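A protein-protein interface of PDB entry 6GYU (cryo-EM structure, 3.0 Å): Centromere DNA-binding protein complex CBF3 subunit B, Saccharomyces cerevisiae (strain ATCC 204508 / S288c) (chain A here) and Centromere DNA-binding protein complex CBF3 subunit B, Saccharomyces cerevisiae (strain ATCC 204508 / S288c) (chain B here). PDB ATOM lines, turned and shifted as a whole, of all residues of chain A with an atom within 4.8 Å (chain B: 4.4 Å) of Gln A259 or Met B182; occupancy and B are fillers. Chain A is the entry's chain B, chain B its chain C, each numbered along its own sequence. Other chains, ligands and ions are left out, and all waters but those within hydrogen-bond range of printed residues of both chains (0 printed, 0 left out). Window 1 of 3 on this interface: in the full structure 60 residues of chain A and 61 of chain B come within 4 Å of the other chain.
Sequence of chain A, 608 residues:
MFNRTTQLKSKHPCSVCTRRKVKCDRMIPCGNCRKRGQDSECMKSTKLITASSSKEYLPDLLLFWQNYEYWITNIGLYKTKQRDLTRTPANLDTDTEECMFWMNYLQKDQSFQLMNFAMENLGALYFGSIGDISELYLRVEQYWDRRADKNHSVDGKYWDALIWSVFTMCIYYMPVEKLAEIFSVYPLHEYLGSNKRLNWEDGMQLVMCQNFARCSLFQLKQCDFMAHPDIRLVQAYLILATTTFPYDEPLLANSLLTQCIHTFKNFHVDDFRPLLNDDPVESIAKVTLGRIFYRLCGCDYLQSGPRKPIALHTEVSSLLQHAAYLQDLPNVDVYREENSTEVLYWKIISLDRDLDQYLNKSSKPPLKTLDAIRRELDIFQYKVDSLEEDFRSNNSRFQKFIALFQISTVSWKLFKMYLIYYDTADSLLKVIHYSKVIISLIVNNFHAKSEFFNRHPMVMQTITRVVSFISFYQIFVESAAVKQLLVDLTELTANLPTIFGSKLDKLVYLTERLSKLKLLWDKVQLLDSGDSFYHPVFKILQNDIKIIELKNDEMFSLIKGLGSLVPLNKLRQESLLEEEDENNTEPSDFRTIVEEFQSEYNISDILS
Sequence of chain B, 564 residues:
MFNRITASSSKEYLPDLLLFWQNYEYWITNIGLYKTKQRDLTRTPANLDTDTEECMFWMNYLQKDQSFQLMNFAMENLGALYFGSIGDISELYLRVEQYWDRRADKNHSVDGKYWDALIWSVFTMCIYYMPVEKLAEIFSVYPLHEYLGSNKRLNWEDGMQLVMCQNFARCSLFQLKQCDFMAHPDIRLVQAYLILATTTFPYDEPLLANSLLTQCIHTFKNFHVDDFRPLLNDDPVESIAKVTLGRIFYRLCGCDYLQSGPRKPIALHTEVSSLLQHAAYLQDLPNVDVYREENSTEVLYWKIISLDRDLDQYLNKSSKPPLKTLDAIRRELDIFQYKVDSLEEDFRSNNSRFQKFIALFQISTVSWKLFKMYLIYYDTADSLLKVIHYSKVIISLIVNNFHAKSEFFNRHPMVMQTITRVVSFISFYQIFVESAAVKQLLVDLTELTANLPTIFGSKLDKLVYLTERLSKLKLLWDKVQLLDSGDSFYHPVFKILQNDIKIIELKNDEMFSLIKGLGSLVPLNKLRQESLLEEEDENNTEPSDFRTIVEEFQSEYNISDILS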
ATOM      1  N   PHE A 225      -3.282 -21.219  -9.035  1.00  0.00           N
ATOM      2  CA  PHE A 225      -4.699 -20.897  -8.931  1.00  0.00           C
ATOM      3  C   PHE A 225      -5.013 -19.452  -9.281  1.00  0.00           C
ATOM      4  O   PHE A 225      -6.172 -19.147  -9.578  1.00  0.00           O
ATOM      5  CB  PHE A 225      -5.207 -21.214  -7.520  1.00  0.00           C
ATOM      6  CG  PHE A 225      -4.648 -20.318  -6.439  1.00  0.00           C
ATOM      7  CD1 PHE A 225      -3.421 -20.584  -5.860  1.00  0.00           C
ATOM      8  CD2 PHE A 225      -5.387 -19.248  -5.959  1.00  0.00           C
ATOM      9  CE1 PHE A 225      -2.922 -19.777  -4.863  1.00  0.00           C
ATOM     10  CE2 PHE A 225      -4.892 -18.439  -4.962  1.00  0.00           C
ATOM     11  CZ  PHE A 225      -3.661 -18.708  -4.413  1.00  0.00           C
ATOM     12  N   MET A 226      -4.027 -18.562  -9.240  1.00  0.00           N
ATOM     13  CA  MET A 226      -4.282 -17.177  -9.596  1.00  0.00           C
ATOM     14  C   MET A 226      -4.431 -17.005 -11.099  1.00  0.00           C
ATOM     15  O   MET A 226      -5.190 -16.143 -11.548  1.00  0.00           O
ATOM     16  CB  MET A 226      -3.164 -16.296  -9.055  1.00  0.00           C
ATOM     17  CG  MET A 226      -3.110 -16.290  -7.545  1.00  0.00           C
ATOM     18  SD  MET A 226      -1.754 -15.309  -6.909  1.00  0.00           S
ATOM     19  CE  MET A 226      -2.343 -13.672  -7.306  1.00  0.00           C
ATOM     20  N   LEU A 233     -11.285 -23.693  -5.746  1.00  0.00           N
ATOM     21  CA  LEU A 233     -10.530 -22.842  -4.828  1.00  0.00           C
ATOM     22  C   LEU A 233     -11.413 -22.319  -3.704  1.00  0.00           C
ATOM     23  O   LEU A 233     -11.035 -22.362  -2.524  1.00  0.00           O
ATOM     24  CB  LEU A 233      -9.917 -21.671  -5.590  1.00  0.00           C
ATOM     25  CG  LEU A 233      -9.256 -20.588  -4.739  1.00  0.00           C
ATOM     26  CD1 LEU A 233      -8.014 -21.096  -4.038  1.00  0.00           C
ATOM     27  CD2 LEU A 233      -8.957 -19.364  -5.582  1.00  0.00           C
ATOM     28  N   LEU A 251      -3.335 -13.308   7.961  1.00  0.00           N
ATOM     29  CA  LEU A 251      -3.071 -12.492   6.784  1.00  0.00           C
ATOM     30  C   LEU A 251      -2.986 -13.310   5.510  1.00  0.00           C
ATOM     31  O   LEU A 251      -3.214 -12.770   4.424  1.00  0.00           O
ATOM     32  CB  LEU A 251      -1.777 -11.688   6.964  1.00  0.00           C
ATOM     33  CG  LEU A 251      -1.872 -10.302   7.612  1.00  0.00           C
ATOM     34  CD1 LEU A 251      -2.274 -10.348   9.071  1.00  0.00           C
ATOM     35  CD2 LEU A 251      -0.544  -9.589   7.474  1.00  0.00           C
ATOM     36  N   LEU A 252      -2.662 -14.599   5.617  1.00  0.00           N
ATOM     37  CA  LEU A 252      -2.774 -15.482   4.466  1.00  0.00           C
ATOM     38  C   LEU A 252      -4.225 -15.832   4.180  1.00  0.00           C
ATOM     39  O   LEU A 252      -4.604 -15.993   3.016  1.00  0.00           O
ATOM     40  CB  LEU A 252      -1.951 -16.748   4.696  1.00  0.00           C
ATOM     41  CG  LEU A 252      -1.922 -17.817   3.606  1.00  0.00           C
ATOM     42  CD1 LEU A 252      -1.376 -17.251   2.318  1.00  0.00           C
ATOM     43  CD2 LEU A 252      -1.079 -18.981   4.066  1.00  0.00           C
ATOM     44  N   SER A 255      -5.877 -12.932   2.167  1.00  0.00           N
ATOM     45  CA  SER A 255      -5.541 -12.904   0.748  1.00  0.00           C
ATOM     46  C   SER A 255      -6.231 -14.031  -0.006  1.00  0.00           C
ATOM     47  O   SER A 255      -6.688 -13.839  -1.139  1.00  0.00           O
ATOM     48  CB  SER A 255      -4.031 -12.990   0.569  1.00  0.00           C
ATOM     49  OG  SER A 255      -3.386 -11.869   1.139  1.00  0.00           O
ATOM     50  N   LEU A 256      -6.319 -15.214   0.608  1.00  0.00           N
ATOM     51  CA  LEU A 256      -7.091 -16.305   0.024  1.00  0.00           C
ATOM     52  C   LEU A 256      -8.570 -15.972  -0.049  1.00  0.00           C
ATOM     53  O   LEU A 256      -9.235 -16.337  -1.020  1.00  0.00           O
ATOM     54  CB  LEU A 256      -6.893 -17.576   0.835  1.00  0.00           C
ATOM     55  CG  LEU A 256      -5.526 -18.227   0.737  1.00  0.00           C
ATOM     56  CD1 LEU A 256      -5.419 -19.259   1.817  1.00  0.00           C
ATOM     57  CD2 LEU A 256      -5.375 -18.867  -0.621  1.00  0.00           C
ATOM     58  N   LEU A 257      -9.096 -15.263   0.947  1.00  0.00           N
ATOM     59  CA  LEU A 257     -10.492 -14.854   0.902  1.00  0.00           C
ATOM     60  C   LEU A 257     -10.729 -13.787  -0.157  1.00  0.00           C
ATOM     61  O   LEU A 257     -11.780 -13.785  -0.804  1.00  0.00           O
ATOM     62  CB  LEU A 257     -10.923 -14.356   2.275  1.00  0.00           C
ATOM     63  CG  LEU A 257     -12.378 -13.944   2.432  1.00  0.00           C
ATOM     64  CD1 LEU A 257     -13.283 -15.124   2.188  1.00  0.00           C
ATOM     65  CD2 LEU A 257     -12.576 -13.400   3.811  1.00  0.00           C
ATOM     66  N   THR A 258      -9.761 -12.891  -0.359  1.00  0.00           N
ATOM     67  CA  THR A 258      -9.853 -11.919  -1.443  1.00  0.00           C
ATOM     68  C   THR A 258      -9.810 -12.609  -2.802  1.00  0.00           C
ATOM     69  O   THR A 258     -10.548 -12.234  -3.721  1.00  0.00           O
ATOM     70  CB  THR A 258      -8.726 -10.896  -1.308  1.00  0.00           C
ATOM     71  OG1 THR A 258      -8.818 -10.262  -0.028  1.00  0.00           O
ATOM     72  CG2 THR A 258      -8.819  -9.833  -2.379  1.00  0.00           C
ATOM     73  N   GLN A 259      -8.987 -13.651  -2.932  1.00  0.00           N
ATOM     74  CA  GLN A 259      -8.992 -14.440  -4.159  1.00  0.00           C
ATOM     75  C   GLN A 259     -10.278 -15.235  -4.326  1.00  0.00           C
ATOM     76  O   GLN A 259     -10.707 -15.469  -5.456  1.00  0.00           O
ATOM     77  CB  GLN A 259      -7.784 -15.369  -4.203  1.00  0.00           C
ATOM     78  CG  GLN A 259      -6.499 -14.641  -4.486  1.00  0.00           C
ATOM     79  CD  GLN A 259      -6.485 -14.061  -5.883  1.00  0.00           C
ATOM     80  OE1 GLN A 259      -6.955 -14.691  -6.829  1.00  0.00           O
ATOM     81  NE2 GLN A 259      -5.957 -12.854  -6.019  1.00  0.00           N
ATOM     82  N   CYS A 260     -10.926 -15.630  -3.233  1.00  0.00           N
ATOM     83  CA  CYS A 260     -12.218 -16.296  -3.357  1.00  0.00           C
ATOM     84  C   CYS A 260     -13.332 -15.328  -3.731  1.00  0.00           C
ATOM     85  O   CYS A 260     -14.279 -15.723  -4.415  1.00  0.00           O
ATOM     86  CB  CYS A 260     -12.570 -17.022  -2.062  1.00  0.00           C
ATOM     87  SG  CYS A 260     -11.541 -18.452  -1.752  1.00  0.00           S
ATOM     88  N   ILE A 261     -13.239 -14.071  -3.298  1.00  0.00           N
ATOM     89  CA  ILE A 261     -14.178 -13.051  -3.761  1.00  0.00           C
ATOM     90  C   ILE A 261     -13.955 -12.761  -5.240  1.00  0.00           C
ATOM     91  O   ILE A 261     -14.912 -12.639  -6.014  1.00  0.00           O
ATOM     92  CB  ILE A 261     -14.048 -11.777  -2.910  1.00  0.00           C
ATOM     93  CG1 ILE A 261     -14.438 -12.046  -1.466  1.00  0.00           C
ATOM     94  CG2 ILE A 261     -14.924 -10.661  -3.446  1.00  0.00           C
ATOM     95  CD1 ILE A 261     -14.045 -10.927  -0.557  1.00  0.00           C
ATOM     96  N   HIS A 262     -12.688 -12.654  -5.653  1.00  0.00           N
ATOM     97  CA  HIS A 262     -12.361 -12.443  -7.061  1.00  0.00           C
ATOM     98  C   HIS A 262     -12.785 -13.624  -7.923  1.00  0.00           C
ATOM     99  O   HIS A 262     -13.215 -13.443  -9.067  1.00  0.00           O
ATOM    100  CB  HIS A 262     -10.864 -12.196  -7.216  1.00  0.00           C
ATOM    101  CG  HIS A 262     -10.414 -12.119  -8.639  1.00  0.00           C
ATOM    102  ND1 HIS A 262     -10.667 -11.030  -9.443  1.00  0.00           N
ATOM    103  CD2 HIS A 262      -9.740 -13.006  -9.408  1.00  0.00           C
ATOM    104  CE1 HIS A 262     -10.160 -11.246 -10.643  1.00  0.00           C
ATOM    105  NE2 HIS A 262      -9.593 -12.439 -10.648  1.00  0.00           N
ATOM    106  N   THR A 263     -12.673 -14.837  -7.391  1.00  0.00           N
ATOM    107  CA  THR A 263     -13.064 -16.023  -8.137  1.00  0.00           C
ATOM    108  C   THR A 263     -14.577 -16.139  -8.220  1.00  0.00           C
ATOM    109  O   THR A 263     -15.119 -16.491  -9.273  1.00  0.00           O
ATOM    110  CB  THR A 263     -12.453 -17.256  -7.478  1.00  0.00           C
ATOM    111  OG1 THR A 263     -11.028 -17.119  -7.450  1.00  0.00           O
ATOM    112  CG2 THR A 263     -12.801 -18.498  -8.242  1.00  0.00           C
ATOM    113  N   ASP B 180       6.067 -15.943  -0.563  1.00  0.00           N
ATOM    114  CA  ASP B 180       4.718 -16.203  -0.056  1.00  0.00           C
ATOM    115  C   ASP B 180       4.004 -14.878   0.216  1.00  0.00           C
ATOM    116  O   ASP B 180       3.656 -14.532   1.343  1.00  0.00           O
ATOM    117  CB  ASP B 180       4.736 -17.110   1.182  1.00  0.00           C
ATOM    118  CG  ASP B 180       5.105 -18.545   0.849  1.00  0.00           C
ATOM    119  OD1 ASP B 180       4.795 -18.993  -0.275  1.00  0.00           O
ATOM    120  OD2 ASP B 180       5.704 -19.228   1.707  1.00  0.00           O
ATOM    121  N   PHE B 181       3.824 -14.137  -0.882  1.00  0.00           N
ATOM    122  CA  PHE B 181       3.381 -12.749  -0.829  1.00  0.00           C
ATOM    123  C   PHE B 181       1.955 -12.606  -0.329  1.00  0.00           C
ATOM    124  O   PHE B 181       1.586 -11.531   0.155  1.00  0.00           O
ATOM    125  CB  PHE B 181       3.515 -12.103  -2.215  1.00  0.00           C
ATOM    126  CG  PHE B 181       2.543 -12.628  -3.246  1.00  0.00           C
ATOM    127  CD1 PHE B 181       2.809 -13.792  -3.944  1.00  0.00           C
ATOM    128  CD2 PHE B 181       1.393 -11.921  -3.557  1.00  0.00           C
ATOM    129  CE1 PHE B 181       1.927 -14.261  -4.894  1.00  0.00           C
ATOM    130  CE2 PHE B 181       0.511 -12.385  -4.503  1.00  0.00           C
ATOM    131  CZ  PHE B 181       0.781 -13.553  -5.175  1.00  0.00           C
ATOM    132  N   MET B 182       1.145 -13.654  -0.449  1.00  0.00           N
ATOM    133  CA  MET B 182      -0.213 -13.609   0.067  1.00  0.00           C
ATOM    134  C   MET B 182      -0.237 -13.636   1.587  1.00  0.00           C
ATOM    135  O   MET B 182      -1.179 -13.122   2.197  1.00  0.00           O
ATOM    136  CB  MET B 182      -1.015 -14.771  -0.509  1.00  0.00           C
ATOM    137  CG  MET B 182      -1.215 -14.656  -2.005  1.00  0.00           C
ATOM    138  SD  MET B 182      -2.075 -16.064  -2.705  1.00  0.00           S
ATOM    139  CE  MET B 182      -3.724 -15.789  -2.077  1.00  0.00           C
ATOM    140  N   ALA B 183       0.785 -14.213   2.212  1.00  0.00           N
ATOM    141  CA  ALA B 183       0.905 -14.182   3.661  1.00  0.00           C
ATOM    142  C   ALA B 183       1.603 -12.930   4.166  1.00  0.00           C
ATOM    143  O   ALA B 183       1.567 -12.663   5.371  1.00  0.00           O
ATOM    144  CB  ALA B 183       1.659 -15.418   4.156  1.00  0.00           C
ATOM    145  N   HIS B 184       2.235 -12.161   3.280  1.00  0.00           N
ATOM    146  CA  HIS B 184       3.000 -10.973   3.655  1.00  0.00           C
ATOM    147  C   HIS B 184       2.674  -9.849   2.681  1.00  0.00           C
ATOM    148  O   HIS B 184       3.398  -9.639   1.700  1.00  0.00           O
ATOM    149  CB  HIS B 184       4.499 -11.267   3.657  1.00  0.00           C
ATOM    150  CG  HIS B 184       4.894 -12.384   4.569  1.00  0.00           C
ATOM    151  ND1 HIS B 184       4.985 -13.691   4.144  1.00  0.00           N
ATOM    152  CD2 HIS B 184       5.196 -12.396   5.888  1.00  0.00           C
ATOM    153  CE1 HIS B 184       5.342 -14.457   5.158  1.00  0.00           C
ATOM    154  NE2 HIS B 184       5.476 -13.696   6.228  1.00  0.00           N
ATOM    155  N   SER B 211      -5.645 -11.334 -11.224  1.00  0.00           N
ATOM    156  CA  SER B 211      -5.474 -11.804  -9.854  1.00  0.00           C
ATOM    157  C   SER B 211      -4.362 -11.045  -9.144  1.00  0.00           C
ATOM    158  O   SER B 211      -4.482 -10.728  -7.953  1.00  0.00           O
ATOM    159  CB  SER B 211      -5.185 -13.300  -9.847  1.00  0.00           C
ATOM    160  OG  SER B 211      -6.278 -14.031 -10.369  1.00  0.00           O
ATOM    161  N   THR B 214      -5.868  -7.746  -8.288  1.00  0.00           N
ATOM    162  CA  THR B 214      -6.720  -7.893  -7.113  1.00  0.00           C
ATOM    163  C   THR B 214      -5.894  -7.972  -5.834  1.00  0.00           C
ATOM    164  O   THR B 214      -6.258  -7.362  -4.820  1.00  0.00           O
ATOM    165  CB  THR B 214      -7.600  -9.131  -7.274  1.00  0.00           C
ATOM    166  OG1 THR B 214      -8.375  -9.006  -8.471  1.00  0.00           O
ATOM    167  CG2 THR B 214      -8.545  -9.289  -6.100  1.00  0.00           C
ATOM    168  N   GLN B 215      -4.756  -8.670  -5.876  1.00  0.00           N
ATOM    169  CA  GLN B 215      -3.854  -8.672  -4.728  1.00  0.00           C
ATOM    170  C   GLN B 215      -3.209  -7.311  -4.502  1.00  0.00           C
ATOM    171  O   GLN B 215      -2.905  -6.962  -3.361  1.00  0.00           O
ATOM    172  CB  GLN B 215      -2.778  -9.739  -4.891  1.00  0.00           C
ATOM    173  CG  GLN B 215      -3.295 -11.146  -4.749  1.00  0.00           C
ATOM    174  CD  GLN B 215      -3.889 -11.397  -3.385  1.00  0.00           C
ATOM    175  OE1 GLN B 215      -5.095 -11.592  -3.245  1.00  0.00           O
ATOM    176  NE2 GLN B 215      -3.046 -11.372  -2.362  1.00  0.00           N
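Of the 8 printed residues of chain B, 6 touch a printed residue of chain A. Printed residues of chain B that touch a printed residue of chain A: Phe B181, Met B182, Ala B183, Ser B211, Thr B214 and Gln B215. Hydrophobic or aromatic side chains of chain B within 4 Å of the printed part of chain A: Phe B181, Met B182 and Ala B183. Among the printed residues, no Asp or Glu carboxylate lies within 4 Å of a Lys or Arg side-chain nitrogen of the other chain.
The side-chain hydroxyl of Ser A255 lies within hydrogen-bond range of the backbone carbonyl oxygen of Leu A251 (3.4 Å). The backbone carbonyl oxygen (O) of Leu A256 sits at hydrogen-bond distance from the side-chain sulfur (SG) of Cys A260, 3.2 Å away. O of Gln A259 lies within hydrogen-bond range of OG1 of Thr A263 (2.6 Å).
Printed residues of chain B within 4 Å of Leu A252: Met B182 and Ala B183. Printed residues of chain B within 4 Å of Leu A256: Met B182. Printed residues of chain B within 4 Å of Thr A258: Thr B214. Gln A259 touches just these residues of chain B: Met B182, Ser B211 and Gln B215. Thr A263 touches none of the printed residues of chain B. Of the printed residues of chain A, Phe B181 touches Met A226. Met B182 touches just these residues of chain A: Phe A225, Leu A251, Leu A252, Ser A255, Leu A256 and Gln A259.
OG of Ser B211 is in hydrogen-bond range of O of Met A226 (2.7 Å). O of Met B182 sits at hydrogen-bond distance from OG of Ser A255 (2.7 Å). The backbone carbonyl oxygen of Ser A255 sits close to the side-chain amide oxygen of Gln B215 (3.5 Å). NE2 of Gln A259 lies within hydrogen-bond range of O of Ser B211 (3.2 Å). The side-chain amide nitrogen of Gln A259 sits at hydrogen-bond distance from the side-chain amide oxygen of Gln B215 (3.2 Å). The side-chain hydroxyl (OG1) of Thr B214 lies within hydrogen-bond range of a ring nitrogen (ND1) of His A262 (3.2 Å). The backbone carbonyl oxygen of Met B182 sits close to the backbone carbonyl oxygen of Leu A251, at 3.0 Å.
Among the printed residues, merely in contact across the chains: Phe A225 with Met B182, Met A226 with Phe B181, Met A226 with Gln B215, Leu A251 with Ala B183, Leu A252 with Met B182, Leu A252 with Ala B183, Leu A256 with Met B182, Thr A258 with Thr B214, Gln A259 with Met B182 and His A262 with Ser B211.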
